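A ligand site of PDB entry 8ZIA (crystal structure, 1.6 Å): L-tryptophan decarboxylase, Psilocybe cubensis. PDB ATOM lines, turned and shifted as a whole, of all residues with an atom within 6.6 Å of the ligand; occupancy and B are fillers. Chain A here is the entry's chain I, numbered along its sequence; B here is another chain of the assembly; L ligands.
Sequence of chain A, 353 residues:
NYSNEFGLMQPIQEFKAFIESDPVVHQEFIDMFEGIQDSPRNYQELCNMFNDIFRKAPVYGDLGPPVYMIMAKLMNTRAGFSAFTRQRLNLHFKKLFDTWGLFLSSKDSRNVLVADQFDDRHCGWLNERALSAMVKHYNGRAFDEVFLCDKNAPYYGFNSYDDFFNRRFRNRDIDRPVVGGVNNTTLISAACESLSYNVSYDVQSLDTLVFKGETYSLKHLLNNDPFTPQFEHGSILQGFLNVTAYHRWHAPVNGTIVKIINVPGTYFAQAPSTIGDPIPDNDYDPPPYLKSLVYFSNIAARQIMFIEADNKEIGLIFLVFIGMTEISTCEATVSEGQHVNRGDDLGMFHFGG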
ATOM      1  N   LEU A  63      14.943 -11.141  -4.249  1.00  0.00           N
ATOM      2  CA  LEU A  63      14.727 -11.610  -2.878  1.00  0.00           C
ATOM      3  C   LEU A  63      14.030 -12.965  -2.848  1.00  0.00           C
ATOM      4  O   LEU A  63      14.317 -13.804  -1.978  1.00  0.00           O
ATOM      5  CB  LEU A  63      13.908 -10.577  -2.111  1.00  0.00           C
ATOM      6  CG  LEU A  63      13.200 -11.162  -0.889  1.00  0.00           C
ATOM      7  CD1 LEU A  63      14.187 -11.279   0.256  1.00  0.00           C
ATOM      8  CD2 LEU A  63      11.981 -10.347  -0.512  1.00  0.00           C
ATOM      9  N   GLY A  64      13.079 -13.174  -3.753  1.00  0.00           N
ATOM     10  CA  GLY A  64      12.349 -14.420  -3.814  1.00  0.00           C
ATOM     11  C   GLY A  64      12.235 -14.908  -5.238  1.00  0.00           C
ATOM     12  O   GLY A  64      12.730 -14.282  -6.185  1.00  0.00           O
ATOM     13  N   PRO A  65      11.592 -16.061  -5.405  1.00  0.00           N
ATOM     14  CA  PRO A  65      11.468 -16.647  -6.738  1.00  0.00           C
ATOM     15  C   PRO A  65      10.512 -15.837  -7.608  1.00  0.00           C
ATOM     16  O   PRO A  65       9.781 -14.962  -7.111  1.00  0.00           O
ATOM     17  CB  PRO A  65      10.941 -18.058  -6.459  1.00  0.00           C
ATOM     18  CG  PRO A  65      10.184 -17.926  -5.153  1.00  0.00           C
ATOM     19  CD  PRO A  65      10.883 -16.830  -4.366  1.00  0.00           C
ATOM     20  N   TYR A  68       6.527 -15.317  -6.883  1.00  0.00           N
ATOM     21  CA  TYR A  68       6.383 -14.449  -5.713  1.00  0.00           C
ATOM     22  C   TYR A  68       6.602 -12.987  -6.089  1.00  0.00           C
ATOM     23  O   TYR A  68       5.826 -12.106  -5.683  1.00  0.00           O
ATOM     24  CB  TYR A  68       7.356 -14.819  -4.591  1.00  0.00           C
ATOM     25  CG  TYR A  68       7.383 -13.702  -3.564  1.00  0.00           C
ATOM     26  CD1 TYR A  68       6.331 -13.542  -2.644  1.00  0.00           C
ATOM     27  CD2 TYR A  68       8.396 -12.753  -3.561  1.00  0.00           C
ATOM     28  CE1 TYR A  68       6.325 -12.509  -1.743  1.00  0.00           C
ATOM     29  CE2 TYR A  68       8.395 -11.701  -2.655  1.00  0.00           C
ATOM     30  CZ  TYR A  68       7.352 -11.580  -1.756  1.00  0.00           C
ATOM     31  OH  TYR A  68       7.341 -10.548  -0.846  1.00  0.00           O
ATOM     32  N   MET A  69       7.667 -12.702  -6.838  1.00  0.00           N
ATOM     33  CA  MET A  69       8.020 -11.307  -7.087  1.00  0.00           C
ATOM     34  C   MET A  69       6.886 -10.544  -7.760  1.00  0.00           C
ATOM     35  O   MET A  69       6.670  -9.367  -7.466  1.00  0.00           O
ATOM     36  CB  MET A  69       9.291 -11.221  -7.929  1.00  0.00           C
ATOM     37  CG  MET A  69      10.548 -11.738  -7.220  1.00  0.00           C
ATOM     38  SD  MET A  69      10.974 -10.921  -5.663  1.00  0.00           S
ATOM     39  CE  MET A  69      11.420  -9.281  -6.224  1.00  0.00           C
ATOM     40  N   PHE A 165      19.118 -27.043  -7.996  1.00  0.00           N
ATOM     41  CA  PHE A 165      18.350 -26.654  -6.818  1.00  0.00           C
ATOM     42  C   PHE A 165      18.485 -27.679  -5.711  1.00  0.00           C
ATOM     43  O   PHE A 165      18.585 -27.330  -4.530  1.00  0.00           O
ATOM     44  CB  PHE A 165      16.886 -26.477  -7.238  1.00  0.00           C
ATOM     45  CG  PHE A 165      16.005 -25.890  -6.189  1.00  0.00           C
ATOM     46  CD1 PHE A 165      16.182 -24.566  -5.787  1.00  0.00           C
ATOM     47  CD2 PHE A 165      14.996 -26.635  -5.619  1.00  0.00           C
ATOM     48  CE1 PHE A 165      15.335 -24.007  -4.800  1.00  0.00           C
ATOM     49  CE2 PHE A 165      14.158 -26.079  -4.629  1.00  0.00           C
ATOM     50  CZ  PHE A 165      14.346 -24.767  -4.232  1.00  0.00           C
ATOM     51  N   PHE A 240      13.396 -20.970   8.128  1.00  0.00           N
ATOM     52  CA  PHE A 240      13.133 -20.426   6.798  1.00  0.00           C
ATOM     53  C   PHE A 240      14.329 -20.732   5.914  1.00  0.00           C
ATOM     54  O   PHE A 240      15.464 -20.380   6.267  1.00  0.00           O
ATOM     55  CB  PHE A 240      12.890 -18.921   6.881  1.00  0.00           C
ATOM     56  CG  PHE A 240      12.983 -18.194   5.573  1.00  0.00           C
ATOM     57  CD1 PHE A 240      12.227 -18.593   4.488  1.00  0.00           C
ATOM     58  CD2 PHE A 240      13.788 -17.065   5.439  1.00  0.00           C
ATOM     59  CE1 PHE A 240      12.302 -17.902   3.282  1.00  0.00           C
ATOM     60  CE2 PHE A 240      13.863 -16.374   4.233  1.00  0.00           C
ATOM     61  CZ  PHE A 240      13.108 -16.786   3.160  1.00  0.00           C
ATOM     62  N   LEU A 241      14.066 -21.377   4.787  1.00  0.00           N
ATOM     63  CA  LEU A 241      15.065 -21.660   3.752  1.00  0.00           C
ATOM     64  C   LEU A 241      14.970 -20.561   2.706  1.00  0.00           C
ATOM     65  O   LEU A 241      13.941 -20.439   2.028  1.00  0.00           O
ATOM     66  CB  LEU A 241      14.799 -23.019   3.093  1.00  0.00           C
ATOM     67  CG  LEU A 241      14.867 -24.350   3.861  1.00  0.00           C
ATOM     68  CD1 LEU A 241      13.675 -24.606   4.781  1.00  0.00           C
ATOM     69  CD2 LEU A 241      15.026 -25.496   2.864  1.00  0.00           C
ATOM     70  N   ASN A 242      16.042 -19.775   2.560  1.00  0.00           N
ATOM     71  CA  ASN A 242      15.993 -18.674   1.607  1.00  0.00           C
ATOM     72  C   ASN A 242      16.361 -19.166   0.205  1.00  0.00           C
ATOM     73  O   ASN A 242      16.655 -20.345  -0.013  1.00  0.00           O
ATOM     74  CB  ASN A 242      16.854 -17.507   2.087  1.00  0.00           C
ATOM     75  CG  ASN A 242      18.337 -17.860   2.200  1.00  0.00           C
ATOM     76  OD1 ASN A 242      18.823 -18.820   1.575  1.00  0.00           O
ATOM     77  ND2 ASN A 242      19.060 -17.087   3.004  1.00  0.00           N
ATOM     78  N   VAL A 243      16.318 -18.251  -0.767  1.00  0.00           N
ATOM     79  CA  VAL A 243      16.414 -18.669  -2.164  1.00  0.00           C
ATOM     80  C   VAL A 243      17.748 -19.330  -2.504  1.00  0.00           C
ATOM     81  O   VAL A 243      17.815 -20.068  -3.492  1.00  0.00           O
ATOM     82  CB  VAL A 243      16.170 -17.480  -3.115  1.00  0.00           C
ATOM     83  CG1 VAL A 243      14.688 -17.121  -3.090  1.00  0.00           C
ATOM     84  CG2 VAL A 243      17.013 -16.291  -2.723  1.00  0.00           C
ATOM     85  N   THR A 244      18.797 -19.099  -1.727  1.00  0.00           N
ATOM     86  CA  THR A 244      20.084 -19.703  -2.032  1.00  0.00           C
ATOM     87  C   THR A 244      20.410 -20.917  -1.163  1.00  0.00           C
ATOM     88  O   THR A 244      21.479 -21.505  -1.335  1.00  0.00           O
ATOM     89  CB  THR A 244      21.211 -18.660  -1.893  1.00  0.00           C
ATOM     90  OG1 THR A 244      21.129 -18.013  -0.622  1.00  0.00           O
ATOM     91  CG2 THR A 244      21.116 -17.620  -3.022  1.00  0.00           C
ATOM     92  N   HIS A 247      18.255 -27.218  -0.338  1.00  0.00           N
ATOM     93  CA  HIS A 247      16.817 -27.420  -0.220  1.00  0.00           C
ATOM     94  C   HIS A 247      16.416 -28.881  -0.057  1.00  0.00           C
ATOM     95  O   HIS A 247      15.229 -29.212  -0.186  1.00  0.00           O
ATOM     96  CB  HIS A 247      16.089 -26.800  -1.422  1.00  0.00           C
ATOM     97  CG  HIS A 247      15.473 -25.467  -1.120  1.00  0.00           C
ATOM     98  ND1 HIS A 247      16.231 -24.329  -0.959  1.00  0.00           N
ATOM     99  CD2 HIS A 247      14.184 -25.103  -0.921  1.00  0.00           C
ATOM    100  CE1 HIS A 247      15.428 -23.299  -0.696  1.00  0.00           C
ATOM    101  NE2 HIS A 247      14.183 -23.752  -0.658  1.00  0.00           N
ATOM    102  N   PRO A 287       9.353  -8.305   3.777  1.00  0.00           N
ATOM    103  CA  PRO A 287       8.002  -7.963   3.337  1.00  0.00           C
ATOM    104  C   PRO A 287       6.969  -8.769   4.095  1.00  0.00           C
ATOM    105  O   PRO A 287       7.311  -9.727   4.805  1.00  0.00           O
ATOM    106  CB  PRO A 287       8.029  -8.346   1.847  1.00  0.00           C
ATOM    107  CG  PRO A 287       8.950  -9.533   1.821  1.00  0.00           C
ATOM    108  CD  PRO A 287      10.035  -9.223   2.851  1.00  0.00           C
ATOM    109  N   TYR A 289       4.771 -11.145   3.454  1.00  0.00           N
ATOM    110  CA  TYR A 289       4.722 -12.604   3.329  1.00  0.00           C
ATOM    111  C   TYR A 289       5.802 -13.261   4.174  1.00  0.00           C
ATOM    112  O   TYR A 289       5.586 -14.324   4.757  1.00  0.00           O
ATOM    113  CB  TYR A 289       4.853 -13.008   1.872  1.00  0.00           C
ATOM    114  CG  TYR A 289       4.752 -14.497   1.581  1.00  0.00           C
ATOM    115  CD1 TYR A 289       3.566 -15.183   1.784  1.00  0.00           C
ATOM    116  CD2 TYR A 289       5.828 -15.197   1.053  1.00  0.00           C
ATOM    117  CE1 TYR A 289       3.453 -16.546   1.505  1.00  0.00           C
ATOM    118  CE2 TYR A 289       5.743 -16.542   0.756  1.00  0.00           C
ATOM    119  CZ  TYR A 289       4.557 -17.210   0.971  1.00  0.00           C
ATOM    120  OH  TYR A 289       4.473 -18.545   0.676  1.00  0.00           O
ATOM    121  N   LEU A 290       6.990 -12.637   4.241  1.00  0.00           N
ATOM    122  CA  LEU A 290       8.066 -13.215   5.054  1.00  0.00           C
ATOM    123  C   LEU A 290       7.905 -12.892   6.536  1.00  0.00           C
ATOM    124  O   LEU A 290       8.732 -13.323   7.335  1.00  0.00           O
ATOM    125  CB  LEU A 290       9.434 -12.734   4.550  1.00  0.00           C
ATOM    126  CG  LEU A 290       9.787 -13.211   3.140  1.00  0.00           C
ATOM    127  CD1 LEU A 290      11.229 -12.880   2.781  1.00  0.00           C
ATOM    128  CD2 LEU A 290       9.512 -14.712   2.970  1.00  0.00           C
ATOM    129  N   GLY A 323       5.307 -25.428   2.145  1.00  0.00           N
ATOM    130  CA  GLY A 323       5.529 -24.759   0.869  1.00  0.00           C
ATOM    131  C   GLY A 323       5.531 -23.249   1.005  1.00  0.00           C
ATOM    132  O   GLY A 323       4.954 -22.658   1.924  1.00  0.00           O
ATOM    133  N   MET A 324       6.198 -22.592   0.062  1.00  0.00           N
ATOM    134  CA  MET A 324       6.122 -21.147  -0.076  1.00  0.00           C
ATOM    135  C   MET A 324       6.032 -20.805  -1.552  1.00  0.00           C
ATOM    136  O   MET A 324       6.919 -21.172  -2.334  1.00  0.00           O
ATOM    137  CB  MET A 324       7.322 -20.458   0.572  1.00  0.00           C
ATOM    138  CG  MET A 324       7.297 -20.551   2.091  1.00  0.00           C
ATOM    139  SD  MET A 324       8.757 -19.852   2.858  1.00  0.00           S
ATOM    140  CE  MET A 324       8.706 -18.155   2.293  1.00  0.00           C
ATOM    141  N   THR A 325       4.962 -20.115  -1.921  1.00  0.00           N
ATOM    142  CA  THR A 325       4.626 -19.782  -3.315  1.00  0.00           C
ATOM    143  C   THR A 325       4.954 -20.949  -4.243  1.00  0.00           C
ATOM    144  O   THR A 325       4.448 -22.059  -4.037  1.00  0.00           O
ATOM    145  CB  THR A 325       5.274 -18.446  -3.738  1.00  0.00           C
ATOM    146  OG1 THR A 325       6.709 -18.501  -3.702  1.00  0.00           O
ATOM    147  CG2 THR A 325       4.823 -17.313  -2.799  1.00  0.00           C
ATOM    148  N   GLU A 326       5.767 -20.725  -5.292  1.00  0.00           N
ATOM    149  CA  GLU A 326       5.993 -21.763  -6.280  1.00  0.00           C
ATOM    150  C   GLU A 326       6.888 -22.894  -5.792  1.00  0.00           C
ATOM    151  O   GLU A 326       6.994 -23.906  -6.490  1.00  0.00           O
ATOM    152  CB  GLU A 326       6.630 -21.165  -7.539  1.00  0.00           C
ATOM    153  CG  GLU A 326       7.936 -20.447  -7.231  1.00  0.00           C
ATOM    154  CD  GLU A 326       7.782 -18.940  -7.271  1.00  0.00           C
ATOM    155  OE1 GLU A 326       7.064 -18.386  -6.420  1.00  0.00           O
ATOM    156  OE2 GLU A 326       8.373 -18.295  -8.165  1.00  0.00           O
ATOM    157  N   ILE A 327       7.539 -22.744  -4.643  1.00  0.00           N
ATOM    158  CA  ILE A 327       8.369 -23.816  -4.107  1.00  0.00           C
ATOM    159  C   ILE A 327       7.555 -24.563  -3.056  1.00  0.00           C
ATOM    160  O   ILE A 327       7.775 -24.424  -1.856  1.00  0.00           O
ATOM    161  CB  ILE A 327       9.689 -23.264  -3.551  1.00  0.00           C
ATOM    162  CG1 ILE A 327      10.366 -22.440  -4.673  1.00  0.00           C
ATOM    163  CG2 ILE A 327      10.588 -24.419  -3.108  1.00  0.00           C
ATOM    164  CD1 ILE A 327      11.703 -21.823  -4.308  1.00  0.00           C
ATOM    165  N   PHE A 349      12.511 -30.297  -1.250  1.00  0.00           N
ATOM    166  CA  PHE A 349      11.562 -29.395  -1.894  1.00  0.00           C
ATOM    167  C   PHE A 349      11.806 -29.367  -3.401  1.00  0.00           C
ATOM    168  O   PHE A 349      12.938 -29.528  -3.867  1.00  0.00           O
ATOM    169  CB  PHE A 349      11.711 -27.971  -1.375  1.00  0.00           C
ATOM    170  CG  PHE A 349      11.267 -27.779   0.047  1.00  0.00           C
ATOM    171  CD1 PHE A 349       9.925 -27.770   0.367  1.00  0.00           C
ATOM    172  CD2 PHE A 349      12.203 -27.533   1.050  1.00  0.00           C
ATOM    173  CE1 PHE A 349       9.512 -27.563   1.671  1.00  0.00           C
ATOM    174  CE2 PHE A 349      11.802 -27.319   2.360  1.00  0.00           C
ATOM    175  CZ  PHE A 349      10.461 -27.342   2.678  1.00  0.00           C
ATOM    176  N   PHE A 351      10.348 -26.871  -6.974  1.00  0.00           N
ATOM    177  CA  PHE A 351       9.377 -26.024  -7.634  1.00  0.00           C
ATOM    178  C   PHE A 351       8.210 -26.895  -8.081  1.00  0.00           C
ATOM    179  O   PHE A 351       8.392 -27.953  -8.683  1.00  0.00           O
ATOM    180  CB  PHE A 351      10.009 -25.329  -8.845  1.00  0.00           C
ATOM    181  CG  PHE A 351      10.841 -24.131  -8.492  1.00  0.00           C
ATOM    182  CD1 PHE A 351      12.071 -24.283  -7.856  1.00  0.00           C
ATOM    183  CD2 PHE A 351      10.426 -22.859  -8.837  1.00  0.00           C
ATOM    184  CE1 PHE A 351      12.842 -23.169  -7.530  1.00  0.00           C
ATOM    185  CE2 PHE A 351      11.192 -21.742  -8.524  1.00  0.00           C
ATOM    186  CZ  PHE A 351      12.412 -21.895  -7.870  1.00  0.00           C
ATOM    187  C   PYR B   1      10.963 -22.939   3.361  1.00  0.00           C
ATOM    188  O   PYR B   1      11.419 -21.807   3.984  1.00  0.00           O
ATOM    189  CA  PYR B   1      10.796 -22.652   1.885  1.00  0.00           C
ATOM    190  O3  PYR B   1      11.396 -21.750   1.387  1.00  0.00           O
ATOM    191  CB  PYR B   1       9.753 -23.472   1.122  1.00  0.00           C
ATOM    192  N   SER B   2       9.976 -23.647   4.093  1.00  0.00           N
ATOM    193  CA  SER B   2      10.012 -23.564   5.542  1.00  0.00           C
ATOM    194  C   SER B   2       9.847 -24.949   6.111  1.00  0.00           C
ATOM    195  O   SER B   2       9.350 -25.850   5.423  1.00  0.00           O
ATOM    196  CB  SER B   2       8.912 -22.614   6.049  1.00  0.00           C
ATOM    197  OG  SER B   2       8.970 -22.455   7.458  1.00  0.00           O
HETATM  198  N1  LIG L   1      12.315 -21.787  -1.067  1.00  0.00           N
HETATM  199  C1  LIG L   1      13.017 -20.574  -1.514  1.00  0.00           C
HETATM  200  C2  LIG L   1      12.554 -19.359  -0.725  1.00  0.00           C
HETATM  201  C3  LIG L   1      11.187 -18.871  -1.085  1.00  0.00           C
HETATM  202  C4  LIG L   1      10.135 -19.569  -1.596  1.00  0.00           C
HETATM  203  N2  LIG L   1       9.056 -18.742  -1.791  1.00  0.00           N
HETATM  204  C5  LIG L   1       9.401 -17.466  -1.403  1.00  0.00           C
HETATM  205  C6  LIG L   1      10.737 -17.501  -0.963  1.00  0.00           C
HETATM  206  C7  LIG L   1       8.660 -16.294  -1.417  1.00  0.00           C
HETATM  207  C8  LIG L   1       9.286 -15.147  -0.974  1.00  0.00           C
HETATM  208  C9  LIG L   1      10.605 -15.158  -0.531  1.00  0.00           C
HETATM  209  C10 LIG L   1      11.337 -16.327  -0.522  1.00  0.00           C
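N of Leu 241 sits at hydrogen-bond distance from O of PYR 1 of chain B, at 2.8 Å. O of His 247 sits at hydrogen-bond distance from N of Phe 349. The backbone NH (N) of Thr 325 is in hydrogen-bond range of the side-chain hydroxyl (OH) of Tyr 289, at 3.1 Å. OE1 of Glu 326 lies within hydrogen-bond range of OG1 of Thr 325, at 2.7 Å. The side-chain carboxylate (OE1) of Glu 326 lies within hydrogen-bond range of the backbone NH (N) of Tyr 68. SD of Met 69 lies within hydrogen-bond range of N of Gly 64, 3.6 Å away. The side-chain amide oxygen (OD1) of Asn 242 lies within hydrogen-bond range of the side-chain hydroxyl (OG1) of Thr 244, 3.3 Å away.
Merely in contact with the ligand: Gly 64 (3.8 Å), Pro 65 (3.4 Å), Tyr 68 (3.5 Å), Leu 241 (3.3 Å), Asn 242 (3.9 Å), Val 243 (3.9 Å), Tyr 289 (3.6 Å), Leu 290 (3.7 Å) and Ile 327 (3.3 Å). Hydrophobic or aromatic side chains that line the ligand: Pro 65, Tyr 68, Val 243, His 247, Tyr 289, Leu 290, Met 324 and Ile 327.
A nitrogen (N1) of the ligand is in hydrogen-bond range of O3 of PYR 1 of chain B. NE2 of His 247 lies within hydrogen-bond range of N1 of the ligand, at 2.7 Å. OG1 of Thr 325 sits at hydrogen-bond distance from N2 of the ligand (3.0 Å). O of Met 324 sits at hydrogen-bond distance from N2 of the ligand (3.3 Å).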
